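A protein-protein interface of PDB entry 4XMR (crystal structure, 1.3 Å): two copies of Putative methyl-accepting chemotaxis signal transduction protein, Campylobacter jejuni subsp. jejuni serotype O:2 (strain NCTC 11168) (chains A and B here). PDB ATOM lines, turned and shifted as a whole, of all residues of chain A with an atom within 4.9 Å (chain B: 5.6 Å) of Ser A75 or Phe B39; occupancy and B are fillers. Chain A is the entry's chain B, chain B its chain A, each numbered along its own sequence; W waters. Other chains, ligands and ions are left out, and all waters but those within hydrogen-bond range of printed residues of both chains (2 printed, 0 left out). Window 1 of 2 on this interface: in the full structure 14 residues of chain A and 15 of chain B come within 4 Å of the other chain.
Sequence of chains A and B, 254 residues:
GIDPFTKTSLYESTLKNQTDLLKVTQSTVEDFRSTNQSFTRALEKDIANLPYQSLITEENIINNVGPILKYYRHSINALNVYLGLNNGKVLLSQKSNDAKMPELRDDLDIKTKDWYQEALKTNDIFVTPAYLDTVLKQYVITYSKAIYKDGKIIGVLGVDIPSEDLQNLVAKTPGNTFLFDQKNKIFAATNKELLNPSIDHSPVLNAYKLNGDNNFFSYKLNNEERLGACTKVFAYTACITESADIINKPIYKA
The side-chain hydroxyl (OG) of Ser B75 lies within hydrogen-bond range of the side-chain hydroxyl (OG) of Ser A75, 3.2 Å away.
O of Ala B42 is in hydrogen-bond range of OH of Tyr B72.
The backbone carbonyl oxygen (O) of Tyr B72 lies within hydrogen-bond range of the side-chain hydroxyl (OG) of Ser B75, 2.7 Å away.
The backbone carbonyl oxygen of Tyr A72 lies within hydrogen-bond range of the side-chain hydroxyl of Ser A75, at 2.7 Å.
Among the printed residues, pairs that only touch across the chains: His A74 with Tyr B72, His A74 with Ala B42, Tyr A72 with Ser B75, Ser A75 with Tyr B72, Tyr A71 with Tyr B72, Ser A75 with Phe B39 and Phe A39 with Ser B75.
Of the printed residues of chain B, Tyr A71 touches Tyr B72 (3.7 Å).
Printed residues of chain B within 4 Å of Tyr A72: Ser B75.
Of the printed residues of chain B, His A74 touches Ala B42 (3.4 Å) and Tyr B72 (3.2 Å).
Of chain B, only Phe B39, Tyr B72 and Ser B75 come within 4 Å of Ser A75.
Asn A77 touches none of the printed residues of chain B.
Of the 8 printed residues of chain A, 5 touch a printed residue of chain B.
Printed residues of chain A that touch a printed residue of chain B: Phe A39, Tyr A71, Tyr A72, His A74 and Ser A75.
Phe A39 touches Ser B75, and with the chains exchanged Ser A75 touches Phe B39.
Tyr A72 touches Ser B75, and with the chains exchanged Ser A75 touches Tyr B72.
Ser B75 touches its own counterpart, Ser A75.
Positions printed for both chains: 39, 72, 73, 75 and 76.
Water W2 bridges the side-chain hydroxyl of Ser B75 and the side-chain hydroxyl of Ser A75.
Water W1 lies within hydrogen-bond range of the backbone carbonyl oxygen of Ala B42 (2.8 Å) and a ring nitrogen (ND1) of His A74 (3.3 Å).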
ATOM      1  N   PHE A  39      -0.772  23.518  -5.022  1.00  0.00           N
ATOM      2  CA  PHE A  39      -1.391  22.300  -5.532  1.00  0.00           C
ATOM      3  C   PHE A  39      -0.497  21.666  -6.597  1.00  0.00           C
ATOM      4  O   PHE A  39      -0.268  20.458  -6.595  1.00  0.00           O
ATOM      5  CB  PHE A  39      -2.759  22.675  -6.115  1.00  0.00           C
ATOM      6  CG  PHE A  39      -3.430  21.589  -6.923  1.00  0.00           C
ATOM      7  CD1 PHE A  39      -4.287  20.684  -6.316  1.00  0.00           C
ATOM      8  CD2 PHE A  39      -3.247  21.511  -8.299  1.00  0.00           C
ATOM      9  CE1 PHE A  39      -4.941  19.712  -7.063  1.00  0.00           C
ATOM     10  CE2 PHE A  39      -3.884  20.535  -9.055  1.00  0.00           C
ATOM     11  CZ  PHE A  39      -4.739  19.640  -8.437  1.00  0.00           C
ATOM     12  N   TYR A  71      -7.080  11.910  -9.285  1.00  0.00           N
ATOM     13  CA  TYR A  71      -7.434  12.201  -7.898  1.00  0.00           C
ATOM     14  C   TYR A  71      -7.129  13.665  -7.592  1.00  0.00           C
ATOM     15  O   TYR A  71      -7.928  14.352  -6.960  1.00  0.00           O
ATOM     16  CB  TYR A  71      -6.716  11.263  -6.918  1.00  0.00           C
ATOM     17  CG  TYR A  71      -7.159   9.824  -7.026  1.00  0.00           C
ATOM     18  CD1 TYR A  71      -8.507   9.497  -7.097  1.00  0.00           C
ATOM     19  CD2 TYR A  71      -6.227   8.791  -7.091  1.00  0.00           C
ATOM     20  CE1 TYR A  71      -8.922   8.158  -7.202  1.00  0.00           C
ATOM     21  CE2 TYR A  71      -6.630   7.468  -7.194  1.00  0.00           C
ATOM     22  CZ  TYR A  71      -7.968   7.147  -7.255  1.00  0.00           C
ATOM     23  OH  TYR A  71      -8.333   5.810  -7.359  1.00  0.00           O
ATOM     24  N   TYR A  72      -5.995  14.162  -8.071  1.00  0.00           N
ATOM     25  CA  TYR A  72      -5.699  15.575  -7.865  1.00  0.00           C
ATOM     26  C   TYR A  72      -6.722  16.477  -8.565  1.00  0.00           C
ATOM     27  O   TYR A  72      -7.200  17.458  -7.989  1.00  0.00           O
ATOM     28  CB  TYR A  72      -4.279  15.903  -8.331  1.00  0.00           C
ATOM     29  CG  TYR A  72      -3.230  15.816  -7.245  1.00  0.00           C
ATOM     30  CD1 TYR A  72      -2.737  14.582  -6.806  1.00  0.00           C
ATOM     31  CD2 TYR A  72      -2.710  16.972  -6.679  1.00  0.00           C
ATOM     32  CE1 TYR A  72      -1.759  14.507  -5.817  1.00  0.00           C
ATOM     33  CE2 TYR A  72      -1.731  16.905  -5.697  1.00  0.00           C
ATOM     34  CZ  TYR A  72      -1.258  15.680  -5.275  1.00  0.00           C
ATOM     35  OH  TYR A  72      -0.279  15.666  -4.305  1.00  0.00           O
ATOM     36  N   ARG A  73      -7.076  16.143  -9.798  1.00  0.00           N
ATOM     37  CA  ARG A  73      -8.078  16.940 -10.510  1.00  0.00           C
ATOM     38  C   ARG A  73      -9.372  17.028  -9.701  1.00  0.00           C
ATOM     39  O   ARG A  73      -9.942  18.108  -9.535  1.00  0.00           O
ATOM     40  CB  ARG A  73      -8.395  16.366 -11.889  1.00  0.00           C
ATOM     41  CG  ARG A  73      -9.496  17.161 -12.597  1.00  0.00           C
ATOM     42  CD  ARG A  73      -9.722  16.758 -14.062  1.00  0.00           C
ATOM     43  NE  ARG A  73     -10.036  15.334 -14.249  1.00  0.00           N
ATOM     44  CZ  ARG A  73     -11.241  14.781 -14.087  1.00  0.00           C
ATOM     45  NH1 ARG A  73     -12.283  15.506 -13.692  1.00  0.00           N
ATOM     46  NH2 ARG A  73     -11.405  13.476 -14.303  1.00  0.00           N
ATOM     47  N   HIS A  74      -9.832  15.889  -9.197  1.00  0.00           N
ATOM     48  CA  HIS A  74     -11.049  15.879  -8.408  1.00  0.00           C
ATOM     49  C   HIS A  74     -10.913  16.693  -7.139  1.00  0.00           C
ATOM     50  O   HIS A  74     -11.858  17.360  -6.723  1.00  0.00           O
ATOM     51  CB  HIS A  74     -11.429  14.454  -8.025  1.00  0.00           C
ATOM     52  CG  HIS A  74     -11.946  13.636  -9.155  1.00  0.00           C
ATOM     53  ND1 HIS A  74     -12.043  12.259  -9.075  1.00  0.00           N
ATOM     54  CD2 HIS A  74     -12.444  13.976 -10.366  1.00  0.00           C
ATOM     55  CE1 HIS A  74     -12.556  11.794 -10.195  1.00  0.00           C
ATOM     56  NE2 HIS A  74     -12.808  12.817 -11.002  1.00  0.00           N
ATOM     57  N   SER A  75      -9.754  16.611  -6.502  1.00  0.00           N
ATOM     58  CA  SER A  75      -9.595  17.252  -5.206  1.00  0.00           C
ATOM     59  C   SER A  75      -9.851  18.762  -5.242  1.00  0.00           C
ATOM     60  O   SER A  75     -10.363  19.314  -4.279  1.00  0.00           O
ATOM     61  CB  SER A  75      -8.230  16.933  -4.594  1.00  0.00           C
ATOM     62  OG  SER A  75      -7.233  17.609  -5.305  1.00  0.00           O
ATOM     63  N   ILE A  76      -9.516  19.396  -6.366  1.00  0.00           N
ATOM     64  CA  ILE A  76      -9.647  20.843  -6.502  1.00  0.00           C
ATOM     65  C   ILE A  76     -10.650  21.242  -7.594  1.00  0.00           C
ATOM     66  O   ILE A  76     -10.871  22.428  -7.837  1.00  0.00           O
ATOM     67  CB  ILE A  76      -8.257  21.501  -6.759  1.00  0.00           C
ATOM     68  CG1 ILE A  76      -8.231  22.977  -6.307  1.00  0.00           C
ATOM     69  CG2 ILE A  76      -7.833  21.329  -8.216  1.00  0.00           C
ATOM     70  CD1 ILE A  76      -6.835  23.597  -6.264  1.00  0.00           C
ATOM     71  N   ASN A  77     -11.263  20.251  -8.241  1.00  0.00           N
ATOM     72  CA  ASN A  77     -12.158  20.488  -9.377  1.00  0.00           C
ATOM     73  C   ASN A  77     -11.469  21.274 -10.503  1.00  0.00           C
ATOM     74  O   ASN A  77     -12.038  22.203 -11.068  1.00  0.00           O
ATOM     75  CB  ASN A  77     -13.466  21.172  -8.941  1.00  0.00           C
ATOM     76  CG  ASN A  77     -14.524  21.140 -10.020  1.00  0.00           C
ATOM     77  OD1 ASN A  77     -14.591  20.195 -10.804  1.00  0.00           O
ATOM     78  ND2 ASN A  77     -15.339  22.186 -10.086  1.00  0.00           N
ATOM     79  N   SER B  34     -16.255  26.085   2.920  1.00  0.00           N
ATOM     80  CA  SER B  34     -16.808  25.483   1.716  1.00  0.00           C
ATOM     81  C   SER B  34     -15.728  24.766   0.928  1.00  0.00           C
ATOM     82  O   SER B  34     -15.978  23.729   0.330  1.00  0.00           O
ATOM     83  CB  SER B  34     -17.482  26.543   0.845  1.00  0.00           C
ATOM     84  OG  SER B  34     -18.444  27.266   1.586  1.00  0.00           O
ATOM     85  N   THR B  35     -14.523  25.320   0.920  1.00  0.00           N
ATOM     86  CA  THR B  35     -13.423  24.674   0.221  1.00  0.00           C
ATOM     87  C   THR B  35     -13.138  23.312   0.848  1.00  0.00           C
ATOM     88  O   THR B  35     -12.933  22.321   0.143  1.00  0.00           O
ATOM     89  CB  THR B  35     -12.186  25.574   0.243  1.00  0.00           C
ATOM     90  OG1 THR B  35     -12.448  26.689  -0.614  1.00  0.00           O
ATOM     91  CG2 THR B  35     -10.946  24.857  -0.261  1.00  0.00           C
ATOM     92  N   ASN B  36     -13.144  23.253   2.170  1.00  0.00           N
ATOM     93  CA  ASN B  36     -12.892  21.996   2.847  1.00  0.00           C
ATOM     94  C   ASN B  36     -14.031  21.009   2.651  1.00  0.00           C
ATOM     95  O   ASN B  36     -13.789  19.800   2.536  1.00  0.00           O
ATOM     96  CB  ASN B  36     -12.616  22.244   4.320  1.00  0.00           C
ATOM     97  CG  ASN B  36     -11.276  22.915   4.539  1.00  0.00           C
ATOM     98  OD1 ASN B  36     -10.356  22.712   3.758  1.00  0.00           O
ATOM     99  ND2 ASN B  36     -11.161  23.728   5.588  1.00  0.00           N
ATOM    100  N   GLN B  37     -15.267  21.504   2.615  1.00  0.00           N
ATOM    101  CA  GLN B  37     -16.406  20.639   2.333  1.00  0.00           C
ATOM    102  C   GLN B  37     -16.357  20.069   0.922  1.00  0.00           C
ATOM    103  O   GLN B  37     -16.611  18.888   0.733  1.00  0.00           O
ATOM    104  CB  GLN B  37     -17.729  21.373   2.573  1.00  0.00           C
ATOM    105  CG  GLN B  37     -18.021  21.667   4.030  1.00  0.00           C
ATOM    106  CD  GLN B  37     -19.151  22.672   4.185  1.00  0.00           C
ATOM    107  OE1 GLN B  37     -19.242  23.642   3.431  1.00  0.00           O
ATOM    108  NE2 GLN B  37     -20.003  22.453   5.175  1.00  0.00           N
ATOM    109  N   SER B  38     -16.036  20.901  -0.064  1.00  0.00           N
ATOM    110  CA  SER B  38     -15.954  20.426  -1.444  1.00  0.00           C
ATOM    111  C   SER B  38     -14.899  19.338  -1.591  1.00  0.00           C
ATOM    112  O   SER B  38     -15.125  18.319  -2.240  1.00  0.00           O
ATOM    113  CB  SER B  38     -15.668  21.590  -2.397  1.00  0.00           C
ATOM    114  OG  SER B  38     -16.770  22.494  -2.430  1.00  0.00           O
ATOM    115  N   PHE B  39     -13.763  19.550  -0.946  1.00  0.00           N
ATOM    116  CA  PHE B  39     -12.667  18.584  -0.936  1.00  0.00           C
ATOM    117  C   PHE B  39     -13.131  17.249  -0.349  1.00  0.00           C
ATOM    118  O   PHE B  39     -12.898  16.180  -0.915  1.00  0.00           O
ATOM    119  CB  PHE B  39     -11.532  19.176  -0.101  1.00  0.00           C
ATOM    120  CG  PHE B  39     -10.404  18.227   0.199  1.00  0.00           C
ATOM    121  CD1 PHE B  39     -10.408  17.480   1.371  1.00  0.00           C
ATOM    122  CD2 PHE B  39      -9.312  18.131  -0.645  1.00  0.00           C
ATOM    123  CE1 PHE B  39      -9.350  16.652   1.678  1.00  0.00           C
ATOM    124  CE2 PHE B  39      -8.242  17.298  -0.331  1.00  0.00           C
ATOM    125  CZ  PHE B  39      -8.267  16.556   0.822  1.00  0.00           C
ATOM    126  N   THR B  40     -13.806  17.327   0.789  1.00  0.00           N
ATOM    127  CA  THR B  40     -14.273  16.135   1.482  1.00  0.00           C
ATOM    128  C   THR B  40     -15.285  15.371   0.633  1.00  0.00           C
ATOM    129  O   THR B  40     -15.259  14.139   0.568  1.00  0.00           O
ATOM    130  CB  THR B  40     -14.854  16.534   2.853  1.00  0.00           C
ATOM    131  OG1 THR B  40     -13.819  17.149   3.638  1.00  0.00           O
ATOM    132  CG2 THR B  40     -15.348  15.318   3.597  1.00  0.00           C
ATOM    133  N   ARG B  41     -16.203  16.102   0.008  1.00  0.00           N
ATOM    134  CA  ARG B  41     -17.195  15.521  -0.883  1.00  0.00           C
ATOM    135  C   ARG B  41     -16.559  14.810  -2.077  1.00  0.00           C
ATOM    136  O   ARG B  41     -16.995  13.725  -2.470  1.00  0.00           O
ATOM    137  CB  ARG B  41     -18.179  16.613  -1.334  1.00  0.00           C
ATOM    138  CG  ARG B  41     -19.209  16.186  -2.374  1.00  0.00           C
ATOM    139  CD  ARG B  41     -20.529  16.958  -2.205  1.00  0.00           C
ATOM    140  NE  ARG B  41     -21.214  16.548  -0.981  1.00  0.00           N
ATOM    141  CZ  ARG B  41     -21.459  17.330   0.066  1.00  0.00           C
ATOM    142  NH1 ARG B  41     -21.118  18.616   0.055  1.00  0.00           N
ATOM    143  NH2 ARG B  41     -22.072  16.820   1.126  1.00  0.00           N
ATOM    144  N   ALA B  42     -15.525  15.415  -2.651  1.00  0.00           N
ATOM    145  CA  ALA B  42     -14.838  14.812  -3.787  1.00  0.00           C
ATOM    146  C   ALA B  42     -14.154  13.511  -3.369  1.00  0.00           C
ATOM    147  O   ALA B  42     -14.200  12.511  -4.099  1.00  0.00           O
ATOM    148  CB  ALA B  42     -13.831  15.787  -4.384  1.00  0.00           C
ATOM    149  N   LEU B  43     -13.552  13.514  -2.184  1.00  0.00           N
ATOM    150  CA  LEU B  43     -12.873  12.332  -1.670  1.00  0.00           C
ATOM    151  C   LEU B  43     -13.891  11.213  -1.406  1.00  0.00           C
ATOM    152  O   LEU B  43     -13.675  10.056  -1.785  1.00  0.00           O
ATOM    153  CB  LEU B  43     -12.092  12.717  -0.409  1.00  0.00           C
ATOM    154  CG  LEU B  43     -11.284  11.605   0.285  1.00  0.00           C
ATOM    155  CD1 LEU B  43     -10.446  10.783  -0.685  1.00  0.00           C
ATOM    156  CD2 LEU B  43     -10.378  12.283   1.311  1.00  0.00           C
ATOM    157  N   GLU B  44     -15.018  11.576  -0.802  1.00  0.00           N
ATOM    158  CA  GLU B  44     -16.100  10.621  -0.593  1.00  0.00           C
ATOM    159  C   GLU B  44     -16.483   9.953  -1.912  1.00  0.00           C
ATOM    160  O   GLU B  44     -16.638   8.731  -1.979  1.00  0.00           O
ATOM    161  CB  GLU B  44     -17.331  11.326  -0.003  1.00  0.00           C
ATOM    162  CG  GLU B  44     -18.628  10.513  -0.123  1.00  0.00           C
ATOM    163  CD  GLU B  44     -19.841  11.299   0.342  1.00  0.00           C
ATOM    164  OE1 GLU B  44     -19.998  12.465  -0.077  1.00  0.00           O
ATOM    165  OE2 GLU B  44     -20.627  10.773   1.146  1.00  0.00           O
ATOM    166  N   TYR B  72      -4.991  13.015  -1.818  1.00  0.00           N
ATOM    167  CA  TYR B  72      -5.857  14.095  -1.375  1.00  0.00           C
ATOM    168  C   TYR B  72      -5.215  14.882  -0.242  1.00  0.00           C
ATOM    169  O   TYR B  72      -5.227  16.112  -0.258  1.00  0.00           O
ATOM    170  CB  TYR B  72      -7.229  13.563  -0.951  1.00  0.00           C
ATOM    171  CG  TYR B  72      -8.272  13.516  -2.049  1.00  0.00           C
ATOM    172  CD1 TYR B  72      -8.224  12.552  -3.053  1.00  0.00           C
ATOM    173  CD2 TYR B  72      -9.321  14.427  -2.071  1.00  0.00           C
ATOM    174  CE1 TYR B  72      -9.189  12.502  -4.055  1.00  0.00           C
ATOM    175  CE2 TYR B  72     -10.281  14.391  -3.064  1.00  0.00           C
ATOM    176  CZ  TYR B  72     -10.233  13.414  -4.037  1.00  0.00           C
ATOM    177  OH  TYR B  72     -11.225  13.401  -4.998  1.00  0.00           O
ATOM    178  N   ARG B  73      -4.610  14.186   0.723  1.00  0.00           N
ATOM    179  CA  ARG B  73      -3.949  14.888   1.812  1.00  0.00           C
ATOM    180  C   ARG B  73      -2.899  15.860   1.274  1.00  0.00           C
ATOM    181  O   ARG B  73      -2.830  17.035   1.676  1.00  0.00           O
ATOM    182  CB  ARG B  73      -3.308  13.918   2.808  1.00  0.00           C
ATOM    183  CG  ARG B  73      -2.531  14.654   3.904  1.00  0.00           C
ATOM    184  CD  ARG B  73      -2.006  13.723   5.003  1.00  0.00           C
ATOM    185  NE  ARG B  73      -1.126  12.647   4.532  1.00  0.00           N
ATOM    186  CZ  ARG B  73       0.178  12.770   4.281  1.00  0.00           C
ATOM    187  NH1 ARG B  73       0.782  13.956   4.376  1.00  0.00           N
ATOM    188  NH2 ARG B  73       0.877  11.705   3.905  1.00  0.00           N
ATOM    189  N   SER B  75      -2.671  17.135  -1.709  1.00  0.00           N
ATOM    190  CA  SER B  75      -3.187  18.155  -2.607  1.00  0.00           C
ATOM    191  C   SER B  75      -3.561  19.437  -1.872  1.00  0.00           C
ATOM    192  O   SER B  75      -3.415  20.526  -2.429  1.00  0.00           O
ATOM    193  CB  SER B  75      -4.368  17.613  -3.410  1.00  0.00           C
ATOM    194  OG  SER B  75      -5.501  17.468  -2.596  1.00  0.00           O
ATOM    195  N   ILE B  76      -4.044  19.332  -0.635  1.00  0.00           N
ATOM    196  CA  ILE B  76      -4.387  20.533   0.133  1.00  0.00           C
ATOM    197  C   ILE B  76      -3.540  20.742   1.372  1.00  0.00           C
ATOM    198  O   ILE B  76      -3.778  21.676   2.141  1.00  0.00           O
ATOM    199  CB  ILE B  76      -5.854  20.545   0.586  1.00  0.00           C
ATOM    200  CG1 ILE B  76      -6.147  19.387   1.541  1.00  0.00           C
ATOM    201  CG2 ILE B  76      -6.758  20.523  -0.600  1.00  0.00           C
ATOM    202  CD1 ILE B  76      -7.439  19.559   2.294  1.00  0.00           C
ATOM    203  N   ALA B  78      -3.419  18.817   4.053  1.00  0.00           N
ATOM    204  CA  ALA B  78      -4.151  18.497   5.278  1.00  0.00           C
ATOM    205  C   ALA B  78      -3.216  17.830   6.278  1.00  0.00           C
ATOM    206  O   ALA B  78      -2.173  17.304   5.903  1.00  0.00           O
ATOM    207  CB  ALA B  78      -5.348  17.596   4.989  1.00  0.00           C
ATOM    208  N   VAL B  81      -5.785  12.520   6.915  1.00  0.00           N
ATOM    209  CA  VAL B  81      -6.945  12.138   6.116  1.00  0.00           C
ATOM    210  C   VAL B  81      -7.128  10.642   6.364  1.00  0.00           C
ATOM    211  O   VAL B  81      -6.151   9.895   6.317  1.00  0.00           O
ATOM    212  CB  VAL B  81      -6.740  12.439   4.612  1.00  0.00           C
ATOM    213  CG1 VAL B  81      -7.925  11.938   3.792  1.00  0.00           C
ATOM    214  CG2 VAL B  81      -6.525  13.930   4.380  1.00  0.00           C
ATOM    215  N   VAL B 159     -11.161  14.371   7.642  1.00  0.00           N
ATOM    216  CA  VAL B 159     -10.140  15.269   7.111  1.00  0.00           C
ATOM    217  C   VAL B 159      -9.819  16.301   8.200  1.00  0.00           C
ATOM    218  O   VAL B 159     -10.714  17.032   8.634  1.00  0.00           O
ATOM    219  CB  VAL B 159     -10.632  16.000   5.832  1.00  0.00           C
ATOM    220  CG1 VAL B 159      -9.589  17.029   5.378  1.00  0.00           C
ATOM    221  CG2 VAL B 159     -10.980  14.999   4.731  1.00  0.00           C
HETATM  222  O   HOH W   1     -14.397  13.030  -6.848  1.00  0.00           O
HETATM  223  O   HOH W   2      -6.920  19.708  -3.405  1.00  0.00           O
